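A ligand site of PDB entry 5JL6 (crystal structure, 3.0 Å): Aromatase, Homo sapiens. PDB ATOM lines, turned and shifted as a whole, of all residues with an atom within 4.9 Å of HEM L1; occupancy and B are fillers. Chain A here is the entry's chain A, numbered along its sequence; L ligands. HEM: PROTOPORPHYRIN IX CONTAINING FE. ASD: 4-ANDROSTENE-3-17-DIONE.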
ATOM      1  N   MET A 107      23.990  10.676  17.855  1.00  0.00           N
ATOM      2  CA  MET A 107      23.244  11.676  18.638  1.00  0.00           C
ATOM      3  C   MET A 107      24.170  12.622  19.404  1.00  0.00           C
ATOM      4  O   MET A 107      23.819  13.783  19.640  1.00  0.00           O
ATOM      5  CB  MET A 107      22.226  10.998  19.570  1.00  0.00           C
ATOM      6  CG  MET A 107      21.202  10.153  18.808  1.00  0.00           C
ATOM      7  SD  MET A 107      19.635   9.734  19.617  1.00  0.00           S
ATOM      8  CE  MET A 107      20.253   9.292  21.223  1.00  0.00           C
ATOM      9  N   ARG A 115      17.682  16.358  10.217  1.00  0.00           N
ATOM     10  CA  ARG A 115      16.840  15.232   9.845  1.00  0.00           C
ATOM     11  C   ARG A 115      16.764  15.190   8.316  1.00  0.00           C
ATOM     12  O   ARG A 115      17.630  15.756   7.637  1.00  0.00           O
ATOM     13  CB  ARG A 115      15.453  15.376  10.493  1.00  0.00           C
ATOM     14  CG  ARG A 115      15.500  15.712  11.964  1.00  0.00           C
ATOM     15  CD  ARG A 115      14.208  15.334  12.682  1.00  0.00           C
ATOM     16  NE  ARG A 115      14.267  15.784  14.066  1.00  0.00           N
ATOM     17  CZ  ARG A 115      14.854  15.133  15.079  1.00  0.00           C
ATOM     18  NH1 ARG A 115      15.424  13.941  14.904  1.00  0.00           N
ATOM     19  NH2 ARG A 115      14.847  15.682  16.285  1.00  0.00           N
ATOM     20  N   ILE A 132      11.166  23.697  14.204  1.00  0.00           N
ATOM     21  CA  ILE A 132      12.384  22.992  14.566  1.00  0.00           C
ATOM     22  C   ILE A 132      12.361  21.492  14.299  1.00  0.00           C
ATOM     23  O   ILE A 132      13.406  20.941  13.993  1.00  0.00           O
ATOM     24  CB  ILE A 132      12.813  23.219  16.021  1.00  0.00           C
ATOM     25  CG1 ILE A 132      11.734  22.810  17.001  1.00  0.00           C
ATOM     26  CG2 ILE A 132      13.185  24.686  16.203  1.00  0.00           C
ATOM     27  CD1 ILE A 132      12.292  22.674  18.395  1.00  0.00           C
ATOM     28  N   ILE A 133      11.199  20.837  14.391  1.00  0.00           N
ATOM     29  CA  ILE A 133      11.166  19.367  14.385  1.00  0.00           C
ATOM     30  C   ILE A 133      11.819  18.826  13.117  1.00  0.00           C
ATOM     31  O   ILE A 133      12.736  18.024  13.211  1.00  0.00           O
ATOM     32  CB  ILE A 133       9.749  18.771  14.519  1.00  0.00           C
ATOM     33  CG1 ILE A 133       9.067  19.228  15.822  1.00  0.00           C
ATOM     34  CG2 ILE A 133       9.825  17.246  14.556  1.00  0.00           C
ATOM     35  CD1 ILE A 133       7.571  19.051  15.793  1.00  0.00           C
ATOM     36  N   TRP A 141      17.654  26.330  12.157  1.00  0.00           N
ATOM     37  CA  TRP A 141      17.401  25.436  13.287  1.00  0.00           C
ATOM     38  C   TRP A 141      18.121  25.909  14.550  1.00  0.00           C
ATOM     39  O   TRP A 141      17.500  26.041  15.603  1.00  0.00           O
ATOM     40  CB  TRP A 141      17.838  24.005  12.955  1.00  0.00           C
ATOM     41  CG  TRP A 141      17.815  23.045  14.121  1.00  0.00           C
ATOM     42  CD1 TRP A 141      16.724  22.459  14.683  1.00  0.00           C
ATOM     43  CD2 TRP A 141      18.948  22.588  14.869  1.00  0.00           C
ATOM     44  NE1 TRP A 141      17.097  21.650  15.728  1.00  0.00           N
ATOM     45  CE2 TRP A 141      18.456  21.711  15.868  1.00  0.00           C
ATOM     46  CE3 TRP A 141      20.325  22.817  14.786  1.00  0.00           C
ATOM     47  CZ2 TRP A 141      19.305  21.082  16.778  1.00  0.00           C
ATOM     48  CZ3 TRP A 141      21.165  22.185  15.691  1.00  0.00           C
ATOM     49  CH2 TRP A 141      20.641  21.323  16.676  1.00  0.00           C
ATOM     50  N   ARG A 145      15.730  26.779  17.966  1.00  0.00           N
ATOM     51  CA  ARG A 145      15.683  25.799  19.049  1.00  0.00           C
ATOM     52  C   ARG A 145      15.735  26.406  20.456  1.00  0.00           C
ATOM     53  O   ARG A 145      14.950  26.012  21.318  1.00  0.00           O
ATOM     54  CB  ARG A 145      16.790  24.753  18.870  1.00  0.00           C
ATOM     55  CG  ARG A 145      16.801  23.667  19.940  1.00  0.00           C
ATOM     56  CD  ARG A 145      17.648  22.475  19.504  1.00  0.00           C
ATOM     57  NE  ARG A 145      17.942  21.567  20.625  1.00  0.00           N
ATOM     58  CZ  ARG A 145      17.329  20.415  20.879  1.00  0.00           C
ATOM     59  NH1 ARG A 145      16.346  19.944  20.127  1.00  0.00           N
ATOM     60  NH2 ARG A 145      17.733  19.706  21.921  1.00  0.00           N
ATOM     61  N   PHE A 148      12.387  27.059  22.132  1.00  0.00           N
ATOM     62  CA  PHE A 148      11.769  25.844  22.619  1.00  0.00           C
ATOM     63  C   PHE A 148      12.434  25.359  23.892  1.00  0.00           C
ATOM     64  O   PHE A 148      11.736  24.963  24.835  1.00  0.00           O
ATOM     65  CB  PHE A 148      11.821  24.732  21.561  1.00  0.00           C
ATOM     66  CG  PHE A 148      10.827  24.918  20.445  1.00  0.00           C
ATOM     67  CD1 PHE A 148      11.138  25.689  19.334  1.00  0.00           C
ATOM     68  CD2 PHE A 148       9.583  24.306  20.516  1.00  0.00           C
ATOM     69  CE1 PHE A 148      10.219  25.848  18.315  1.00  0.00           C
ATOM     70  CE2 PHE A 148       8.663  24.465  19.498  1.00  0.00           C
ATOM     71  CZ  PHE A 148       8.983  25.229  18.396  1.00  0.00           C
ATOM     72  N   LEU A 152      10.597  24.945  27.779  1.00  0.00           N
ATOM     73  CA  LEU A 152      10.402  23.571  28.262  1.00  0.00           C
ATOM     74  C   LEU A 152      11.313  23.192  29.445  1.00  0.00           C
ATOM     75  O   LEU A 152      11.560  22.011  29.688  1.00  0.00           O
ATOM     76  CB  LEU A 152      10.640  22.601  27.097  1.00  0.00           C
ATOM     77  CG  LEU A 152       9.713  22.761  25.882  1.00  0.00           C
ATOM     78  CD1 LEU A 152      10.214  21.948  24.704  1.00  0.00           C
ATOM     79  CD2 LEU A 152       8.300  22.344  26.238  1.00  0.00           C
ATOM     80  N   PHE A 203       2.100  27.697  27.056  1.00  0.00           N
ATOM     81  CA  PHE A 203       2.920  28.281  25.970  1.00  0.00           C
ATOM     82  C   PHE A 203       2.271  29.417  25.168  1.00  0.00           C
ATOM     83  O   PHE A 203       2.988  30.139  24.473  1.00  0.00           O
ATOM     84  CB  PHE A 203       3.332  27.183  24.989  1.00  0.00           C
ATOM     85  CG  PHE A 203       4.032  26.024  25.631  1.00  0.00           C
ATOM     86  CD1 PHE A 203       5.240  26.199  26.297  1.00  0.00           C
ATOM     87  CD2 PHE A 203       3.496  24.745  25.563  1.00  0.00           C
ATOM     88  CE1 PHE A 203       5.884  25.125  26.888  1.00  0.00           C
ATOM     89  CE2 PHE A 203       4.146  23.667  26.146  1.00  0.00           C
ATOM     90  CZ  PHE A 203       5.335  23.865  26.815  1.00  0.00           C
ATOM     91  N   MET A 303       4.673  23.664  18.845  1.00  0.00           N
ATOM     92  CA  MET A 303       4.585  23.492  20.313  1.00  0.00           C
ATOM     93  C   MET A 303       3.228  22.946  20.767  1.00  0.00           C
ATOM     94  O   MET A 303       3.162  22.128  21.683  1.00  0.00           O
ATOM     95  CB  MET A 303       4.897  24.819  21.022  1.00  0.00           C
ATOM     96  CG  MET A 303       5.125  24.694  22.524  1.00  0.00           C
ATOM     97  SD  MET A 303       6.655  23.854  22.978  1.00  0.00           S
ATOM     98  CE  MET A 303       7.768  25.242  23.188  1.00  0.00           C
ATOM     99  N   ALA A 306       2.740  19.057  19.779  1.00  0.00           N
ATOM    100  CA  ALA A 306       3.754  18.119  20.266  1.00  0.00           C
ATOM    101  C   ALA A 306       3.218  17.116  21.261  1.00  0.00           C
ATOM    102  O   ALA A 306       3.377  15.906  21.094  1.00  0.00           O
ATOM    103  CB  ALA A 306       4.940  18.867  20.870  1.00  0.00           C
ATOM    104  N   ALA A 307       2.586  17.646  22.305  1.00  0.00           N
ATOM    105  CA  ALA A 307       2.086  16.794  23.376  1.00  0.00           C
ATOM    106  C   ALA A 307       0.896  15.937  22.913  1.00  0.00           C
ATOM    107  O   ALA A 307       0.924  14.716  23.065  1.00  0.00           O
ATOM    108  CB  ALA A 307       1.776  17.617  24.631  1.00  0.00           C
ATOM    109  N   THR A 310       2.095  12.859  20.886  1.00  0.00           N
ATOM    110  CA  THR A 310       3.000  11.871  21.458  1.00  0.00           C
ATOM    111  C   THR A 310       2.696  11.446  22.902  1.00  0.00           C
ATOM    112  O   THR A 310       2.793  10.264  23.218  1.00  0.00           O
ATOM    113  CB  THR A 310       4.432  12.395  21.380  1.00  0.00           C
ATOM    114  OG1 THR A 310       4.524  13.665  22.056  1.00  0.00           O
ATOM    115  CG2 THR A 310       4.824  12.560  19.926  1.00  0.00           C
ATOM    116  N   MET A 311       2.361  12.386  23.766  1.00  0.00           N
ATOM    117  CA  MET A 311       2.031  12.067  25.155  1.00  0.00           C
ATOM    118  C   MET A 311       0.739  11.288  25.252  1.00  0.00           C
ATOM    119  O   MET A 311       0.644  10.321  26.007  1.00  0.00           O
ATOM    120  CB  MET A 311       1.831  13.338  25.980  1.00  0.00           C
ATOM    121  CG  MET A 311       3.086  14.176  26.136  1.00  0.00           C
ATOM    122  SD  MET A 311       4.069  13.712  27.546  1.00  0.00           S
ATOM    123  CE  MET A 311       2.950  14.232  28.840  1.00  0.00           C
ATOM    124  N   SER A 314       1.303   7.767  24.230  1.00  0.00           N
ATOM    125  CA  SER A 314       2.203   7.146  25.219  1.00  0.00           C
ATOM    126  C   SER A 314       1.474   6.779  26.511  1.00  0.00           C
ATOM    127  O   SER A 314       1.634   5.679  27.030  1.00  0.00           O
ATOM    128  CB  SER A 314       3.386   8.059  25.549  1.00  0.00           C
ATOM    129  OG  SER A 314       4.210   8.250  24.415  1.00  0.00           O
ATOM    130  N   MET A 364       7.755   2.974  27.947  1.00  0.00           N
ATOM    131  CA  MET A 364       8.373   3.548  26.740  1.00  0.00           C
ATOM    132  C   MET A 364       9.382   2.601  26.095  1.00  0.00           C
ATOM    133  O   MET A 364       9.504   2.610  24.880  1.00  0.00           O
ATOM    134  CB  MET A 364       9.088   4.848  27.063  1.00  0.00           C
ATOM    135  CG  MET A 364       8.181   5.971  27.520  1.00  0.00           C
ATOM    136  SD  MET A 364       9.161   7.360  28.117  1.00  0.00           S
ATOM    137  CE  MET A 364       9.522   8.050  26.529  1.00  0.00           C
ATOM    138  N   VAL A 370       7.531   6.635  19.889  1.00  0.00           N
ATOM    139  CA  VAL A 370       8.587   7.179  19.046  1.00  0.00           C
ATOM    140  C   VAL A 370       9.697   6.132  19.021  1.00  0.00           C
ATOM    141  O   VAL A 370      10.683   6.210  19.750  1.00  0.00           O
ATOM    142  CB  VAL A 370       9.078   8.544  19.554  1.00  0.00           C
ATOM    143  CG1 VAL A 370       9.979   9.201  18.521  1.00  0.00           C
ATOM    144  CG2 VAL A 370       7.893   9.449  19.881  1.00  0.00           C
ATOM    145  N   VAL A 373      14.095   7.457  14.922  1.00  0.00           N
ATOM    146  CA  VAL A 373      14.586   8.830  14.866  1.00  0.00           C
ATOM    147  C   VAL A 373      15.295   9.024  13.544  1.00  0.00           C
ATOM    148  O   VAL A 373      16.151   8.215  13.182  1.00  0.00           O
ATOM    149  CB  VAL A 373      15.601   9.097  15.992  1.00  0.00           C
ATOM    150  CG1 VAL A 373      16.164  10.503  15.888  1.00  0.00           C
ATOM    151  CG2 VAL A 373      14.961   8.843  17.347  1.00  0.00           C
ATOM    152  N   ARG A 375      17.808  11.162  11.252  1.00  0.00           N
ATOM    153  CA  ARG A 375      18.918  12.124  11.259  1.00  0.00           C
ATOM    154  C   ARG A 375      19.612  12.188   9.902  1.00  0.00           C
ATOM    155  O   ARG A 375      19.268  11.455   8.974  1.00  0.00           O
ATOM    156  CB  ARG A 375      19.930  11.765  12.343  1.00  0.00           C
ATOM    157  CG  ARG A 375      19.358  11.752  13.751  1.00  0.00           C
ATOM    158  CD  ARG A 375      18.778  13.089  14.193  1.00  0.00           C
ATOM    159  NE  ARG A 375      18.846  13.268  15.639  1.00  0.00           N
ATOM    160  CZ  ARG A 375      19.944  13.615  16.318  1.00  0.00           C
ATOM    161  NH1 ARG A 375      21.097  13.807  15.682  1.00  0.00           N
ATOM    162  NH2 ARG A 375      19.887  13.771  17.635  1.00  0.00           N
ATOM    163  N   ILE A 398      15.549   2.982  17.503  1.00  0.00           N
ATOM    164  CA  ILE A 398      15.741   2.873  18.949  1.00  0.00           C
ATOM    165  C   ILE A 398      14.797   1.853  19.596  1.00  0.00           C
ATOM    166  O   ILE A 398      15.127   1.306  20.653  1.00  0.00           O
ATOM    167  CB  ILE A 398      15.644   4.225  19.685  1.00  0.00           C
ATOM    168  CG1 ILE A 398      14.279   4.894  19.504  1.00  0.00           C
ATOM    169  CG2 ILE A 398      16.744   5.159  19.214  1.00  0.00           C
ATOM    170  CD1 ILE A 398      13.957   5.899  20.587  1.00  0.00           C
ATOM    171  N   PRO A 429      15.088   6.796  25.058  1.00  0.00           N
ATOM    172  CA  PRO A 429      13.719   6.913  24.582  1.00  0.00           C
ATOM    173  C   PRO A 429      13.377   8.309  24.036  1.00  0.00           C
ATOM    174  O   PRO A 429      12.442   8.448  23.247  1.00  0.00           O
ATOM    175  CB  PRO A 429      12.894   6.627  25.839  1.00  0.00           C
ATOM    176  CG  PRO A 429      13.739   7.137  26.945  1.00  0.00           C
ATOM    177  CD  PRO A 429      15.143   6.844  26.533  1.00  0.00           C
ATOM    178  N   PHE A 430      14.118   9.326  24.486  1.00  0.00           N
ATOM    179  CA  PHE A 430      13.932  10.696  24.036  1.00  0.00           C
ATOM    180  C   PHE A 430      15.038  11.174  23.103  1.00  0.00           C
ATOM    181  O   PHE A 430      14.921  12.251  22.533  1.00  0.00           O
ATOM    182  CB  PHE A 430      13.927  11.642  25.230  1.00  0.00           C
ATOM    183  CG  PHE A 430      12.782  11.432  26.186  1.00  0.00           C
ATOM    184  CD1 PHE A 430      13.009  11.030  27.491  1.00  0.00           C
ATOM    185  CD2 PHE A 430      11.485  11.691  25.789  1.00  0.00           C
ATOM    186  CE1 PHE A 430      11.967  10.856  28.380  1.00  0.00           C
ATOM    187  CE2 PHE A 430      10.429  11.537  26.673  1.00  0.00           C
ATOM    188  CZ  PHE A 430      10.666  11.109  27.971  1.00  0.00           C
ATOM    189  N   GLY A 431      16.130  10.431  22.971  1.00  0.00           N
ATOM    190  CA  GLY A 431      17.366  10.969  22.396  1.00  0.00           C
ATOM    191  C   GLY A 431      18.075  11.932  23.362  1.00  0.00           C
ATOM    192  O   GLY A 431      17.535  12.278  24.413  1.00  0.00           O
ATOM    193  N   PHE A 432      19.287  12.350  22.996  1.00  0.00           N
ATOM    194  CA  PHE A 432      20.073  13.313  23.781  1.00  0.00           C
ATOM    195  C   PHE A 432      20.964  14.130  22.843  1.00  0.00           C
ATOM    196  O   PHE A 432      20.915  13.967  21.605  1.00  0.00           O
ATOM    197  CB  PHE A 432      20.910  12.617  24.869  1.00  0.00           C
ATOM    198  CG  PHE A 432      22.122  11.891  24.319  1.00  0.00           C
ATOM    199  CD1 PHE A 432      23.382  12.449  24.386  1.00  0.00           C
ATOM    200  CD2 PHE A 432      21.964  10.663  23.709  1.00  0.00           C
ATOM    201  CE1 PHE A 432      24.470  11.781  23.845  1.00  0.00           C
ATOM    202  CE2 PHE A 432      23.043   9.983  23.169  1.00  0.00           C
ATOM    203  CZ  PHE A 432      24.303  10.551  23.231  1.00  0.00           C
ATOM    204  N   ARG A 435      20.530  17.798  19.492  1.00  0.00           N
ATOM    205  CA  ARG A 435      19.211  17.689  18.852  1.00  0.00           C
ATOM    206  C   ARG A 435      18.323  16.608  19.487  1.00  0.00           C
ATOM    207  O   ARG A 435      17.425  16.076  18.831  1.00  0.00           O
ATOM    208  CB  ARG A 435      19.391  17.411  17.353  1.00  0.00           C
ATOM    209  CG  ARG A 435      18.090  17.497  16.567  1.00  0.00           C
ATOM    210  CD  ARG A 435      18.260  18.114  15.200  1.00  0.00           C
ATOM    211  NE  ARG A 435      16.965  18.582  14.729  1.00  0.00           N
ATOM    212  CZ  ARG A 435      16.765  19.268  13.609  1.00  0.00           C
ATOM    213  NH1 ARG A 435      17.781  19.569  12.795  1.00  0.00           N
ATOM    214  NH2 ARG A 435      15.537  19.645  13.286  1.00  0.00           N
ATOM    215  N   GLY A 436      18.552  16.301  20.759  1.00  0.00           N
ATOM    216  CA  GLY A 436      17.665  15.425  21.512  1.00  0.00           C
ATOM    217  C   GLY A 436      16.311  16.082  21.689  1.00  0.00           C
ATOM    218  O   GLY A 436      16.122  17.234  21.317  1.00  0.00           O
ATOM    219  N   CYS A 437      15.362  15.337  22.238  1.00  0.00           N
ATOM    220  CA  CYS A 437      14.008  15.853  22.445  1.00  0.00           C
ATOM    221  C   CYS A 437      14.019  17.092  23.327  1.00  0.00           C
ATOM    222  O   CYS A 437      14.586  17.066  24.406  1.00  0.00           O
ATOM    223  CB  CYS A 437      13.134  14.771  23.076  1.00  0.00           C
ATOM    224  SG  CYS A 437      11.457  15.286  23.452  1.00  0.00           S
ATOM    225  N   ALA A 438      13.433  18.177  22.844  1.00  0.00           N
ATOM    226  CA  ALA A 438      13.358  19.416  23.621  1.00  0.00           C
ATOM    227  C   ALA A 438      12.422  19.274  24.815  1.00  0.00           C
ATOM    228  O   ALA A 438      12.572  19.976  25.803  1.00  0.00           O
ATOM    229  CB  ALA A 438      12.911  20.575  22.743  1.00  0.00           C
ATOM    230  N   GLY A 439      11.446  18.378  24.708  1.00  0.00           N
ATOM    231  CA  GLY A 439      10.503  18.151  25.798  1.00  0.00           C
ATOM    232  C   GLY A 439      10.925  17.137  26.834  1.00  0.00           C
ATOM    233  O   GLY A 439      10.185  16.897  27.776  1.00  0.00           O
ATOM    234  N   ALA A 443       8.462  16.362  29.742  1.00  0.00           N
ATOM    235  CA  ALA A 443       7.584  15.254  29.365  1.00  0.00           C
ATOM    236  C   ALA A 443       7.409  14.293  30.513  1.00  0.00           C
ATOM    237  O   ALA A 443       6.300  13.902  30.841  1.00  0.00           O
ATOM    238  CB  ALA A 443       8.127  14.532  28.143  1.00  0.00           C
ATOM    239  N   MET A 446       5.219  15.861  33.038  1.00  0.00           N
ATOM    240  CA  MET A 446       3.813  15.848  32.617  1.00  0.00           C
ATOM    241  C   MET A 446       3.187  14.463  32.722  1.00  0.00           C
ATOM    242  O   MET A 446       2.040  14.351  33.159  1.00  0.00           O
ATOM    243  CB  MET A 446       3.675  16.358  31.187  1.00  0.00           C
ATOM    244  CG  MET A 446       3.782  17.867  31.044  1.00  0.00           C
ATOM    245  SD  MET A 446       3.330  18.370  29.371  1.00  0.00           S
ATOM    246  CE  MET A 446       4.719  17.752  28.446  1.00  0.00           C
ATOM    247  N   MET A 447       3.914  13.414  32.333  1.00  0.00           N
ATOM    248  CA  MET A 447       3.396  12.037  32.425  1.00  0.00           C
ATOM    249  C   MET A 447       3.141  11.592  33.871  1.00  0.00           C
ATOM    250  O   MET A 447       2.130  10.931  34.124  1.00  0.00           O
ATOM    251  CB  MET A 447       4.324  11.034  31.719  1.00  0.00           C
ATOM    252  CG  MET A 447       4.201  11.142  30.201  1.00  0.00           C
ATOM    253  SD  MET A 447       4.957   9.822  29.249  1.00  0.00           S
ATOM    254  CE  MET A 447       6.655  10.420  29.148  1.00  0.00           C
HETATM  255  CHA HEM L   1      12.124  15.413  19.258  1.00  0.00           C
HETATM  256  CHB HEM L   1      10.527  11.700  21.865  1.00  0.00           C
HETATM  257  CHC HEM L   1       7.347  14.608  24.054  1.00  0.00           C
HETATM  258  CHD HEM L   1       9.098  18.341  21.635  1.00  0.00           C
HETATM  259  C1A HEM L   1      11.975  14.174  19.805  1.00  0.00           C
HETATM  260  C2A HEM L   1      12.758  13.048  19.463  1.00  0.00           C
HETATM  261  C3A HEM L   1      12.313  12.008  20.201  1.00  0.00           C
HETATM  262  C4A HEM L   1      11.260  12.478  21.013  1.00  0.00           C
HETATM  263  CMA HEM L   1      12.888  10.602  20.134  1.00  0.00           C
HETATM  264  CAA HEM L   1      13.902  12.993  18.469  1.00  0.00           C
HETATM  265  CBA HEM L   1      15.166  13.490  19.192  1.00  0.00           C
HETATM  266  CGA HEM L   1      16.418  13.145  18.418  1.00  0.00           C
HETATM  267  O1A HEM L   1      16.465  13.264  17.180  1.00  0.00           O
HETATM  268  O2A HEM L   1      17.432  12.758  19.021  1.00  0.00           O
HETATM  269  C1B HEM L   1       9.480  12.166  22.669  1.00  0.00           C
HETATM  270  C2B HEM L   1       8.713  11.334  23.526  1.00  0.00           C
HETATM  271  C3B HEM L   1       7.804  12.134  24.164  1.00  0.00           C
HETATM  272  C4B HEM L   1       8.060  13.498  23.635  1.00  0.00           C
HETATM  273  CMB HEM L   1       8.927   9.849  23.679  1.00  0.00           C
HETATM  274  CAB HEM L   1       6.755  11.836  25.185  1.00  0.00           C
HETATM  275  CBB HEM L   1       6.474  10.659  25.710  1.00  0.00           C
HETATM  276  C1C HEM L   1       7.557  15.901  23.632  1.00  0.00           C
HETATM  277  C2C HEM L   1       6.876  17.049  24.104  1.00  0.00           C
HETATM  278  C3C HEM L   1       7.390  18.145  23.407  1.00  0.00           C
HETATM  279  C4C HEM L   1       8.371  17.613  22.518  1.00  0.00           C
HETATM  280  CMC HEM L   1       5.830  17.050  25.185  1.00  0.00           C
HETATM  281  CAC HEM L   1       7.031  19.602  23.495  1.00  0.00           C
HETATM  282  CBC HEM L   1       6.088  20.129  24.283  1.00  0.00           C
HETATM  283  C1D HEM L   1      10.043  17.783  20.787  1.00  0.00           C
HETATM  284  C2D HEM L   1      10.746  18.626  19.821  1.00  0.00           C
HETATM  285  C3D HEM L   1      11.596  17.842  19.151  1.00  0.00           C
HETATM  286  C4D HEM L   1      11.389  16.487  19.718  1.00  0.00           C
HETATM  287  CMD HEM L   1      10.569  20.108  19.615  1.00  0.00           C
HETATM  288  CAD HEM L   1      12.514  18.255  18.031  1.00  0.00           C
HETATM  289  CBD HEM L   1      13.917  18.625  18.494  1.00  0.00           C
HETATM  290  CGD HEM L   1      14.757  19.033  17.302  1.00  0.00           C
HETATM  291  O1D HEM L   1      15.606  19.936  17.430  1.00  0.00           O
HETATM  292  O2D HEM L   1      14.613  18.466  16.202  1.00  0.00           O
HETATM  293  NA  HEM L   1      11.073  13.808  20.773  1.00  0.00           N
HETATM  294  NB  HEM L   1       9.070  13.422  22.784  1.00  0.00           N
HETATM  295  NC  HEM L   1       8.449  16.266  22.685  1.00  0.00           N
HETATM  296  ND  HEM L   1      10.466  16.500  20.705  1.00  0.00           N
HETATM  297 FE   HEM L   1       9.816  15.026  21.705  1.00  0.00          FE
HETATM  298  C1  ASD L   2       7.929  15.491  17.669  1.00  0.00           C
HETATM  299  C10 ASD L   2       7.884  13.965  17.439  1.00  0.00           C
HETATM  300  C11 ASD L   2      10.311  14.115  16.519  1.00  0.00           C
HETATM  301  C12 ASD L   2      11.307  13.674  15.455  1.00  0.00           C
HETATM  302  C13 ASD L   2      11.194  12.180  15.206  1.00  0.00           C
HETATM  303  C14 ASD L   2       9.776  11.927  14.753  1.00  0.00           C
HETATM  304  C15 ASD L   2       9.814  10.559  14.078  1.00  0.00           C
HETATM  305  C16 ASD L   2      11.155  10.529  13.346  1.00  0.00           C
HETATM  306  C17 ASD L   2      11.934  11.628  14.023  1.00  0.00           C
HETATM  307  C18 ASD L   2      11.657  11.351  16.406  1.00  0.00           C
HETATM  308  C19 ASD L   2       8.243  13.277  18.748  1.00  0.00           C
HETATM  309  C2  ASD L   2       6.689  16.108  18.292  1.00  0.00           C
HETATM  310  C3  ASD L   2       5.445  15.623  17.614  1.00  0.00           C
HETATM  311  C4  ASD L   2       5.403  14.272  17.021  1.00  0.00           C
HETATM  312  C5  ASD L   2       6.507  13.495  16.977  1.00  0.00           C
HETATM  313  C6  ASD L   2       6.358  12.094  16.444  1.00  0.00           C
HETATM  314  C7  ASD L   2       7.374  11.841  15.352  1.00  0.00           C
HETATM  315  C8  ASD L   2       8.774  12.161  15.850  1.00  0.00           C
HETATM  316  C9  ASD L   2       8.860  13.634  16.284  1.00  0.00           C
HETATM  317  O1  ASD L   2       4.477  16.357  17.521  1.00  0.00           O
HETATM  318  O2  ASD L   2      13.027  12.011  13.638  1.00  0.00           O
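An oxygen (O2A) of HEM L1 sits close to the side-chain sulfur of Met 107. CD1 of Ile 132 touches CMD of HEM L1 (3.3 Å). Ile 133 touches HEM L1. CD2 of Leu 152 touches CBC of HEM L1, at 3.7 Å. Met 303 touches HEM L1. Ala 306 touches HEM L1 (CB to CAC, 3.4 Å). Thr 310 touches HEM L1. Ser 314 touches HEM L1 (OG to CBB, 3.6 Å). CE of Met 364 touches CMB of HEM L1 (3.4 Å). Val 370 touches HEM L1. CG1 of Val 373 touches O1A of HEM L1, at 3.1 Å. O of Pro 429 touches CMB of HEM L1 (3.8 Å). O of Phe 430 touches C3A of HEM L1, at 3.5 Å. Gly 431 touches HEM L1 (CA to O2A, 3.8 Å). Gly 436 touches HEM L1 (CA to O2A, 3.7 Å). Ala 438 touches HEM L1. Gly 439 touches HEM L1 (N to C4C, 3.9 Å). Met 446 touches HEM L1. CE of Met 447 touches CBB of HEM L1 (3.5 Å). Hydrophobic or aromatic side chains within 4 Å of HEM L1: Met 107, Ile 132, Trp 141, Leu 152, Met 303, Ala 306, Met 364, Val 370, Val 373, Phe 430, Ala 438, Met 446 and Met 447. Within 4 Å of HEM L1: Met 107, Arg 115, Ile 132, Ile 133, Trp 141, Arg 145, Leu 152, Met 303, Ala 306, Thr 310, Ser 314, Met 364, Val 370, Val 373, Arg 375, Pro 429, Phe 430, Gly 431, Arg 435, Gly 436, Cys 437, Ala 438, Gly 439, Met 446 and Met 447. Along chain A the residues within 4 Å of HEM L1 span positions 107 to 447.
An oxygen (O2D) of HEM L1 is in salt-bridge range of the guanidinium group of Arg 435 (2.8 Å). The guanidinium group (NH1) of Arg 115 is in salt-bridge range of an oxygen (O1A) of HEM L1 (2.6 Å). An iron atom (FE) of HEM L1 is bound by the side-chain sulfur (SG) of Cys 437, at 2.4 Å. The guanidinium group (NH1) of Arg 115 is in hydrogen-bond range of an oxygen (O2) of ASD L2, 3.3 Å away. The guanidinium group of Arg 145 lies within salt-bridge range of an oxygen (O1D) of HEM L1 (2.8 Å). O1D of HEM L1 sits at hydrogen-bond distance from NE1 of Trp 141 (2.8 Å). O1A of HEM L1 lies within salt-bridge range of NE of Arg 375 (2.8 Å).
O of Ile 132 is in hydrogen-bond range of NH2 of Arg 435, 2.6 Å away. The guanidinium group (NH1) of Arg 145 lies within hydrogen-bond range of the backbone carbonyl oxygen (O) of Gly 436 (3.0 Å). O of Thr 310 lies within hydrogen-bond range of OG of Ser 314 (2.7 Å). O of Ile 133 sits at hydrogen-bond distance from NH2 of Arg 435, at 3.2 Å. The side-chain sulfur (SG) of Cys 437 sits close to the backbone NH (N) of Gly 439, 3.3 Å away. The backbone carbonyl oxygen of Ile 133 sits at hydrogen-bond distance from the guanidinium group of Arg 115, at 2.8 Å. O of Ala 306 is in hydrogen-bond range of OG1 of Thr 310, 2.7 Å away. The backbone NH (N) of Cys 437 is in hydrogen-bond range of the backbone carbonyl oxygen (O) of Phe 430.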
